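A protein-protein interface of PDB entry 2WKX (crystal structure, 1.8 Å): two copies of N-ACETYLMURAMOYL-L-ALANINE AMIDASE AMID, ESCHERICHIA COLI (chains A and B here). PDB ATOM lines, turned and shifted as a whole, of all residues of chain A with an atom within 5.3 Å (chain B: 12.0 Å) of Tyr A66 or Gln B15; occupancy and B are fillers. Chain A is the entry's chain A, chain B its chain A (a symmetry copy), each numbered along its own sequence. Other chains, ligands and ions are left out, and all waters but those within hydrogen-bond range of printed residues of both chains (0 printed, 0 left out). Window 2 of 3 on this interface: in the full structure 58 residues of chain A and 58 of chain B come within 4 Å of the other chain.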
ATOM      1  N   PRO A  64     -19.056 -34.198 -23.386  1.00  0.00           N
ATOM      2  CA  PRO A  64     -18.062 -34.263 -22.311  1.00  0.00           C
ATOM      3  C   PRO A  64     -18.799 -34.556 -21.007  1.00  0.00           C
ATOM      4  O   PRO A  64     -19.930 -34.104 -20.824  1.00  0.00           O
ATOM      5  CB  PRO A  64     -17.456 -32.853 -22.301  1.00  0.00           C
ATOM      6  CG  PRO A  64     -18.532 -31.976 -22.853  1.00  0.00           C
ATOM      7  CD  PRO A  64     -19.266 -32.819 -23.870  1.00  0.00           C
ATOM      8  N   ARG A  65     -18.169 -35.317 -20.119  1.00  0.00           N
ATOM      9  CA  ARG A  65     -18.773 -35.655 -18.826  1.00  0.00           C
ATOM     10  C   ARG A  65     -18.139 -34.884 -17.664  1.00  0.00           C
ATOM     11  O   ARG A  65     -16.912 -34.858 -17.517  1.00  0.00           O
ATOM     12  CB  ARG A  65     -18.720 -37.167 -18.583  1.00  0.00           C
ATOM     13  CG  ARG A  65     -19.359 -37.967 -19.726  1.00  0.00           C
ATOM     14  CD  ARG A  65     -19.278 -39.476 -19.519  1.00  0.00           C
ATOM     15  NE  ARG A  65     -20.195 -39.916 -18.466  1.00  0.00           N
ATOM     16  CZ  ARG A  65     -21.510 -40.061 -18.629  1.00  0.00           C
ATOM     17  NH1 ARG A  65     -22.083 -39.809 -19.805  1.00  0.00           N
ATOM     18  NH2 ARG A  65     -22.262 -40.461 -17.611  1.00  0.00           N
ATOM     19  N   TYR A  66     -19.000 -34.247 -16.871  1.00  0.00           N
ATOM     20  CA  TYR A  66     -18.629 -33.541 -15.646  1.00  0.00           C
ATOM     21  C   TYR A  66     -19.634 -33.943 -14.586  1.00  0.00           C
ATOM     22  O   TYR A  66     -20.839 -34.000 -14.871  1.00  0.00           O
ATOM     23  CB  TYR A  66     -18.715 -32.024 -15.820  1.00  0.00           C
ATOM     24  CG  TYR A  66     -17.906 -31.480 -16.966  1.00  0.00           C
ATOM     25  CD1 TYR A  66     -18.495 -31.271 -18.212  1.00  0.00           C
ATOM     26  CD2 TYR A  66     -16.550 -31.178 -16.806  1.00  0.00           C
ATOM     27  CE1 TYR A  66     -17.761 -30.773 -19.269  1.00  0.00           C
ATOM     28  CE2 TYR A  66     -15.799 -30.682 -17.870  1.00  0.00           C
ATOM     29  CZ  TYR A  66     -16.422 -30.477 -19.093  1.00  0.00           C
ATOM     30  OH  TYR A  66     -15.703 -29.991 -20.154  1.00  0.00           O
ATOM     31  N   ASN A  67     -19.148 -34.204 -13.374  1.00  0.00           N
ATOM     32  CA  ASN A  67     -20.010 -34.631 -12.268  1.00  0.00           C
ATOM     33  C   ASN A  67     -20.735 -35.942 -12.573  1.00  0.00           C
ATOM     34  O   ASN A  67     -21.860 -36.151 -12.114  1.00  0.00           O
ATOM     35  CB  ASN A  67     -21.030 -33.535 -11.921  1.00  0.00           C
ATOM     36  CG  ASN A  67     -20.773 -32.894 -10.575  1.00  0.00           C
ATOM     37  OD1 ASN A  67     -20.195 -33.506  -9.672  1.00  0.00           O
ATOM     38  ND2 ASN A  67     -21.226 -31.650 -10.425  1.00  0.00           N
ATOM     39  N   GLY A  68     -20.082 -36.803 -13.351  1.00  0.00           N
ATOM     40  CA  GLY A  68     -20.659 -38.068 -13.810  1.00  0.00           C
ATOM     41  C   GLY A  68     -21.814 -37.939 -14.795  1.00  0.00           C
ATOM     42  O   GLY A  68     -22.591 -38.883 -14.972  1.00  0.00           O
ATOM     43  N   LYS A  69     -21.934 -36.781 -15.449  1.00  0.00           N
ATOM     44  CA  LYS A  69     -23.064 -36.523 -16.350  1.00  0.00           C
ATOM     45  C   LYS A  69     -22.604 -35.911 -17.662  1.00  0.00           C
ATOM     46  O   LYS A  69     -21.694 -35.077 -17.642  1.00  0.00           O
ATOM     47  CB  LYS A  69     -24.058 -35.533 -15.725  1.00  0.00           C
ATOM     48  CG  LYS A  69     -24.587 -35.897 -14.345  1.00  0.00           C
ATOM     49  CD  LYS A  69     -25.522 -34.809 -13.864  1.00  0.00           C
ATOM     50  CE  LYS A  69     -25.963 -35.112 -12.460  1.00  0.00           C
ATOM     51  NZ  LYS A  69     -26.729 -33.950 -11.969  1.00  0.00           N
ATOM     52  N   PRO A  70     -23.251 -36.289 -18.796  1.00  0.00           N
ATOM     53  CA  PRO A  70     -22.961 -35.649 -20.091  1.00  0.00           C
ATOM     54  C   PRO A  70     -23.423 -34.187 -20.103  1.00  0.00           C
ATOM     55  O   PRO A  70     -24.499 -33.881 -19.568  1.00  0.00           O
ATOM     56  CB  PRO A  70     -23.794 -36.467 -21.097  1.00  0.00           C
ATOM     57  CG  PRO A  70     -24.928 -37.050 -20.295  1.00  0.00           C
ATOM     58  CD  PRO A  70     -24.300 -37.322 -18.915  1.00  0.00           C
ATOM     59  N   ARG A  71     -22.626 -33.299 -20.695  1.00  0.00           N
ATOM     60  CA  ARG A  71     -22.993 -31.884 -20.814  1.00  0.00           C
ATOM     61  C   ARG A  71     -23.647 -31.600 -22.166  1.00  0.00           C
ATOM     62  O   ARG A  71     -23.117 -31.992 -23.221  1.00  0.00           O
ATOM     63  CB  ARG A  71     -21.767 -30.979 -20.622  1.00  0.00           C
ATOM     64  CG  ARG A  71     -22.065 -29.483 -20.708  1.00  0.00           C
ATOM     65  CD  ARG A  71     -20.833 -28.645 -20.347  1.00  0.00           C
ATOM     66  NE  ARG A  71     -20.621 -28.656 -18.906  1.00  0.00           N
ATOM     67  CZ  ARG A  71     -19.639 -28.002 -18.282  1.00  0.00           C
ATOM     68  NH1 ARG A  71     -18.772 -27.267 -18.970  1.00  0.00           N
ATOM     69  NH2 ARG A  71     -19.518 -28.088 -16.966  1.00  0.00           N
ATOM     70  N   ILE A  72     -24.792 -30.920 -22.100  1.00  0.00           N
ATOM     71  CA  ILE A  72     -25.567 -30.479 -23.266  1.00  0.00           C
ATOM     72  C   ILE A  72     -25.676 -28.948 -23.222  1.00  0.00           C
ATOM     73  O   ILE A  72     -25.822 -28.378 -22.137  1.00  0.00           O
ATOM     74  CB  ILE A  72     -26.987 -31.154 -23.281  1.00  0.00           C
ATOM     75  CG1 ILE A  72     -26.893 -32.678 -23.490  1.00  0.00           C
ATOM     76  CG2 ILE A  72     -27.910 -30.551 -24.363  1.00  0.00           C
ATOM     77  CD1 ILE A  72     -28.218 -33.442 -23.142  1.00  0.00           C
ATOM     78  N   GLU B   5     -20.795 -24.758 -12.011  1.00  0.00           N
ATOM     79  CA  GLU B   5     -20.426 -23.312 -11.904  1.00  0.00           C
ATOM     80  C   GLU B   5     -21.581 -22.409 -12.367  1.00  0.00           C
ATOM     81  O   GLU B   5     -22.718 -22.876 -12.533  1.00  0.00           O
ATOM     82  CB  GLU B   5     -19.162 -23.015 -12.726  1.00  0.00           C
ATOM     83  CG  GLU B   5     -18.115 -24.126 -12.752  1.00  0.00           C
ATOM     84  CD  GLU B   5     -16.751 -23.666 -13.257  1.00  0.00           C
ATOM     85  OE1 GLU B   5     -16.252 -22.610 -12.805  1.00  0.00           O
ATOM     86  OE2 GLU B   5     -16.167 -24.373 -14.104  1.00  0.00           O
ATOM     87  N   LYS B   6     -21.283 -21.121 -12.567  1.00  0.00           N
ATOM     88  CA  LYS B   6     -22.231 -20.173 -13.148  1.00  0.00           C
ATOM     89  C   LYS B   6     -22.516 -20.581 -14.598  1.00  0.00           C
ATOM     90  O   LYS B   6     -21.586 -20.834 -15.371  1.00  0.00           O
ATOM     91  CB  LYS B   6     -21.674 -18.748 -13.103  1.00  0.00           C
ATOM     92  CG  LYS B   6     -22.666 -17.670 -13.536  1.00  0.00           C
ATOM     93  CD  LYS B   6     -21.953 -16.503 -14.217  1.00  0.00           C
ATOM     94  CE  LYS B   6     -22.860 -15.291 -14.397  1.00  0.00           C
ATOM     95  NZ  LYS B   6     -23.860 -15.496 -15.479  1.00  0.00           N
ATOM     96  N   GLY B   7     -23.798 -20.643 -14.951  1.00  0.00           N
ATOM     97  CA  GLY B   7     -24.220 -21.048 -16.293  1.00  0.00           C
ATOM     98  C   GLY B   7     -24.278 -22.555 -16.508  1.00  0.00           C
ATOM     99  O   GLY B   7     -24.455 -23.018 -17.640  1.00  0.00           O
ATOM    100  N   ILE B   8     -24.121 -23.320 -15.429  1.00  0.00           N
ATOM    101  CA  ILE B   8     -24.243 -24.779 -15.469  1.00  0.00           C
ATOM    102  C   ILE B   8     -25.441 -25.185 -14.612  1.00  0.00           C
ATOM    103  O   ILE B   8     -25.509 -24.850 -13.426  1.00  0.00           O
ATOM    104  CB  ILE B   8     -22.954 -25.530 -14.995  1.00  0.00           C
ATOM    105  CG1 ILE B   8     -21.713 -25.114 -15.805  1.00  0.00           C
ATOM    106  CG2 ILE B   8     -23.156 -27.054 -15.036  1.00  0.00           C
ATOM    107  CD1 ILE B   8     -21.824 -25.234 -17.335  1.00  0.00           C
ATOM    108  N   VAL B   9     -26.384 -25.890 -15.229  1.00  0.00           N
ATOM    109  CA  VAL B   9     -27.597 -26.340 -14.552  1.00  0.00           C
ATOM    110  C   VAL B   9     -27.538 -27.866 -14.441  1.00  0.00           C
ATOM    111  O   VAL B   9     -27.416 -28.565 -15.460  1.00  0.00           O
ATOM    112  CB  VAL B   9     -28.879 -25.862 -15.287  1.00  0.00           C
ATOM    113  CG1 VAL B   9     -30.140 -26.387 -14.586  1.00  0.00           C
ATOM    114  CG2 VAL B   9     -28.913 -24.336 -15.356  1.00  0.00           C
ATOM    115  N   GLU B  10     -27.599 -28.362 -13.204  1.00  0.00           N
ATOM    116  CA  GLU B  10     -27.558 -29.805 -12.958  1.00  0.00           C
ATOM    117  C   GLU B  10     -28.943 -30.413 -13.151  1.00  0.00           C
ATOM    118  O   GLU B  10     -29.914 -29.904 -12.601  1.00  0.00           O
ATOM    119  CB  GLU B  10     -27.059 -30.109 -11.541  1.00  0.00           C
ATOM    120  CG  GLU B  10     -25.650 -29.602 -11.218  1.00  0.00           C
ATOM    121  CD  GLU B  10     -24.543 -30.318 -11.985  1.00  0.00           C
ATOM    122  OE1 GLU B  10     -23.385 -29.852 -11.932  1.00  0.00           O
ATOM    123  OE2 GLU B  10     -24.817 -31.344 -12.642  1.00  0.00           O
ATOM    124  N   LYS B  11     -29.025 -31.488 -13.937  1.00  0.00           N
ATOM    125  CA  LYS B  11     -30.273 -32.218 -14.147  1.00  0.00           C
ATOM    126  C   LYS B  11     -30.051 -33.697 -13.846  1.00  0.00           C
ATOM    127  O   LYS B  11     -28.932 -34.117 -13.520  1.00  0.00           O
ATOM    128  CB  LYS B  11     -30.785 -32.027 -15.587  1.00  0.00           C
ATOM    129  CG  LYS B  11     -31.233 -30.603 -15.931  1.00  0.00           C
ATOM    130  CD  LYS B  11     -32.500 -30.219 -15.201  1.00  0.00           C
ATOM    131  CE  LYS B  11     -33.035 -28.876 -15.670  1.00  0.00           C
ATOM    132  NZ  LYS B  11     -34.361 -28.579 -15.075  1.00  0.00           N
ATOM    133  N   GLU B  12     -31.112 -34.493 -13.953  1.00  0.00           N
ATOM    134  CA  GLU B  12     -30.984 -35.932 -13.739  1.00  0.00           C
ATOM    135  C   GLU B  12     -30.565 -36.624 -15.038  1.00  0.00           C
ATOM    136  O   GLU B  12     -31.336 -36.689 -16.004  1.00  0.00           O
ATOM    137  CB  GLU B  12     -32.276 -36.531 -13.180  1.00  0.00           C
ATOM    138  CG  GLU B  12     -32.191 -38.028 -12.947  1.00  0.00           C
ATOM    139  CD  GLU B  12     -33.086 -38.489 -11.824  1.00  0.00           C
ATOM    140  OE1 GLU B  12     -32.692 -38.317 -10.648  1.00  0.00           O
ATOM    141  OE2 GLU B  12     -34.174 -39.029 -12.122  1.00  0.00           O
ATOM    142  N   GLY B  13     -29.337 -37.140 -15.041  1.00  0.00           N
ATOM    143  CA  GLY B  13     -28.793 -37.833 -16.199  1.00  0.00           C
ATOM    144  C   GLY B  13     -28.048 -36.958 -17.197  1.00  0.00           C
ATOM    145  O   GLY B  13     -27.538 -37.477 -18.183  1.00  0.00           O
ATOM    146  N   TYR B  14     -27.991 -35.647 -16.954  1.00  0.00           N
ATOM    147  CA  TYR B  14     -27.260 -34.707 -17.818  1.00  0.00           C
ATOM    148  C   TYR B  14     -27.103 -33.359 -17.113  1.00  0.00           C
ATOM    149  O   TYR B  14     -27.766 -33.093 -16.102  1.00  0.00           O
ATOM    150  CB  TYR B  14     -27.957 -34.495 -19.187  1.00  0.00           C
ATOM    151  CG  TYR B  14     -29.339 -33.869 -19.085  1.00  0.00           C
ATOM    152  CD1 TYR B  14     -29.535 -32.506 -19.339  1.00  0.00           C
ATOM    153  CD2 TYR B  14     -30.436 -34.634 -18.683  1.00  0.00           C
ATOM    154  CE1 TYR B  14     -30.827 -31.916 -19.235  1.00  0.00           C
ATOM    155  CE2 TYR B  14     -31.709 -34.064 -18.562  1.00  0.00           C
ATOM    156  CZ  TYR B  14     -31.895 -32.710 -18.834  1.00  0.00           C
ATOM    157  OH  TYR B  14     -33.146 -32.145 -18.722  1.00  0.00           O
ATOM    158  N   GLN B  15     -26.233 -32.503 -17.642  1.00  0.00           N
ATOM    159  CA  GLN B  15     -26.211 -31.110 -17.207  1.00  0.00           C
ATOM    160  C   GLN B  15     -26.352 -30.162 -18.394  1.00  0.00           C
ATOM    161  O   GLN B  15     -26.025 -30.532 -19.540  1.00  0.00           O
ATOM    162  CB  GLN B  15     -24.975 -30.797 -16.359  1.00  0.00           C
ATOM    163  CG  GLN B  15     -23.676 -30.998 -17.064  1.00  0.00           C
ATOM    164  CD  GLN B  15     -22.455 -30.536 -16.257  1.00  0.00           C
ATOM    165  OE1 GLN B  15     -21.481 -30.106 -16.861  1.00  0.00           O
ATOM    166  NE2 GLN B  15     -22.490 -30.642 -14.929  1.00  0.00           N
ATOM    167  N   LEU B  16     -26.838 -28.949 -18.122  1.00  0.00           N
ATOM    168  CA  LEU B  16     -27.015 -27.950 -19.179  1.00  0.00           C
ATOM    169  C   LEU B  16     -26.032 -26.798 -19.032  1.00  0.00           C
ATOM    170  O   LEU B  16     -25.887 -26.219 -17.954  1.00  0.00           O
ATOM    171  CB  LEU B  16     -28.453 -27.397 -19.224  1.00  0.00           C
ATOM    172  CG  LEU B  16     -29.515 -28.424 -19.591  1.00  0.00           C
ATOM    173  CD1 LEU B  16     -30.898 -27.808 -19.362  1.00  0.00           C
ATOM    174  CD2 LEU B  16     -29.332 -28.918 -21.034  1.00  0.00           C
ATOM    175  N   ASP B  17     -25.365 -26.477 -20.138  1.00  0.00           N
ATOM    176  CA  ASP B  17     -24.479 -25.328 -20.194  1.00  0.00           C
ATOM    177  C   ASP B  17     -25.240 -24.181 -20.880  1.00  0.00           C
ATOM    178  O   ASP B  17     -25.546 -24.235 -22.081  1.00  0.00           O
ATOM    179  CB  ASP B  17     -23.202 -25.724 -20.940  1.00  0.00           C
ATOM    180  CG  ASP B  17     -22.128 -24.660 -20.885  1.00  0.00           C
ATOM    181  OD1 ASP B  17     -22.450 -23.458 -20.753  1.00  0.00           O
ATOM    182  OD2 ASP B  17     -20.947 -25.046 -20.992  1.00  0.00           O
ATOM    183  N   THR B  18     -25.552 -23.132 -20.122  1.00  0.00           N
ATOM    184  CA  THR B  18     -26.387 -22.025 -20.622  1.00  0.00           C
ATOM    185  C   THR B  18     -25.572 -20.765 -20.938  1.00  0.00           C
ATOM    186  O   THR B  18     -26.152 -19.684 -21.123  1.00  0.00           O
ATOM    187  CB  THR B  18     -27.474 -21.615 -19.599  1.00  0.00           C
ATOM    188  OG1 THR B  18     -26.840 -21.200 -18.373  1.00  0.00           O
ATOM    189  CG2 THR B  18     -28.469 -22.734 -19.358  1.00  0.00           C
ATOM    190  N   ARG B  19     -24.246 -20.905 -21.000  1.00  0.00           N
ATOM    191  CA  ARG B  19     -23.351 -19.743 -21.111  1.00  0.00           C
ATOM    192  C   ARG B  19     -23.391 -19.010 -22.448  1.00  0.00           C
ATOM    193  O   ARG B  19     -23.118 -17.811 -22.512  1.00  0.00           O
ATOM    194  CB  ARG B  19     -21.910 -20.145 -20.795  1.00  0.00           C
ATOM    195  CG  ARG B  19     -21.667 -20.441 -19.331  1.00  0.00           C
ATOM    196  CD  ARG B  19     -20.371 -21.219 -19.191  1.00  0.00           C
ATOM    197  NE  ARG B  19     -20.024 -21.421 -17.790  1.00  0.00           N
ATOM    198  CZ  ARG B  19     -19.219 -22.382 -17.344  1.00  0.00           C
ATOM    199  NH1 ARG B  19     -18.672 -23.258 -18.184  1.00  0.00           N
ATOM    200  NH2 ARG B  19     -18.973 -22.472 -16.043  1.00  0.00           N
ATOM    201  N   ARG B  20     -23.726 -19.737 -23.509  1.00  0.00           N
ATOM    202  CA  ARG B  20     -23.837 -19.166 -24.840  1.00  0.00           C
ATOM    203  C   ARG B  20     -25.307 -19.005 -25.214  1.00  0.00           C
ATOM    204  O   ARG B  20     -26.022 -20.002 -25.363  1.00  0.00           O
ATOM    205  CB  ARG B  20     -23.104 -20.051 -25.855  1.00  0.00           C
ATOM    206  CG  ARG B  20     -21.580 -20.161 -25.630  1.00  0.00           C
ATOM    207  CD  ARG B  20     -20.856 -18.828 -25.893  1.00  0.00           C
ATOM    208  NE  ARG B  20     -21.384 -18.188 -27.105  1.00  0.00           N
ATOM    209  CZ  ARG B  20     -20.996 -18.472 -28.349  1.00  0.00           C
ATOM    210  NH1 ARG B  20     -20.046 -19.374 -28.578  1.00  0.00           N
ATOM    211  NH2 ARG B  20     -21.556 -17.842 -29.378  1.00  0.00           N
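Tyr A66 touches one residue of chain B.
Gln B15 touches just these residues of chain A: Tyr A66 (3.5 Å), Pro A70 (2.9 Å), Arg A71 (2.7 Å) and Ile A72 (2.9 Å).
No residue of chain B comes within 4 Å of Pro A64.
Asn A67 touches just one residue of chain B: Glu B10 (3.2 Å).
No residue of chain B comes within 4 Å of Gly A68.
Lys A69 touches just these residues of chain B: Glu B10 (3.3 Å), Lys B11 (2.7 Å) and Tyr B14 (3.6 Å).
Printed residues of chain B within 4 Å of Pro A70: Gly B13 (3.3 Å), Tyr B14 (3.4 Å) and Gln B15 (2.9 Å).
Of chain B, only Ile B8, Gln B15 and Asp B17 come within 4 Å of Arg A71.
Of the printed residues of chain A, Lys B11 touches Lys A69 (2.7 Å).
Printed residues of chain A within 4 Å of Leu B16: Ile A72.
Of the printed residues of chain A, Ile B8 touches Arg A71 (3.7 Å).
Gly B7 touches none of the printed residues of chain A.
The nearest residue of chain B that does not touch Tyr A66 is Glu B10 (5.3 Å).
The nearest printed residue of chain A that does not touch Gly B13 is Lys A69 (4.5 Å).
O of Pro A64 is in hydrogen-bond range of N of Arg A71.
The backbone NH (N) of Leu B16 lies within hydrogen-bond range of the backbone carbonyl oxygen (O) of Val B9 (2.8 Å).
NE2 of Gln B15 is in hydrogen-bond range of OE1 of Glu B10 (3.2 Å).
OD1 of Asp B17 sits at hydrogen-bond distance from N of Arg B19, at 3.1 Å.
No position is printed for both chains.
Of the 14 pairs that touch across the chains among the printed residues, none has its exchanged pair printed and touching as well.
The side-chain amide nitrogen (ND2) of Asn A67 is in hydrogen-bond range of the side-chain carboxylate (OE1) of Glu B10, 3.2 Å away.
NZ of Lys A69 lies within salt-bridge range of OE2 of Glu B10, at 3.3 Å.
The side-chain amino group of Lys A69 lies within hydrogen-bond range of the backbone carbonyl oxygen of Lys B11.
The backbone carbonyl oxygen of Pro A70 sits at hydrogen-bond distance from the backbone NH of Gln B15 (2.9 Å).
NE of Arg A71 sits at hydrogen-bond distance from OE1 of Gln B15 (2.7 Å).
The guanidinium group (NH1) of Arg A71 is in salt-bridge range of the side-chain carboxylate (OD2) of Asp B17 (3.7 Å).
The backbone carbonyl oxygen (O) of Gln B15 lies within hydrogen-bond range of the backbone NH (N) of Ile A72, 2.9 Å away.
The backbone carbonyl oxygen (O) of Ile A72 lies within hydrogen-bond range of the backbone NH (N) of Asp B17.
Among the printed residues, merely in contact across the chains: Tyr A66 with Gln B15 (3.5 Å), Lys A69 with Tyr B14 (3.6 Å), Pro A70 with Gly B13 (3.3 Å), Pro A70 with Tyr B14 (3.4 Å), Arg A71 with Ile B8 (3.7 Å) and Ile A72 with Leu B16 (3.2 Å).
Hydrophobic or aromatic side chains of chain B within 4 Å of the printed part of chain A: Ile B8, Tyr B14 and Leu B16.
Printed residues of chain A that touch a printed residue of chain B: Tyr A66, Asn A67, Lys A69, Pro A70, Arg A71 and Ile A72.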
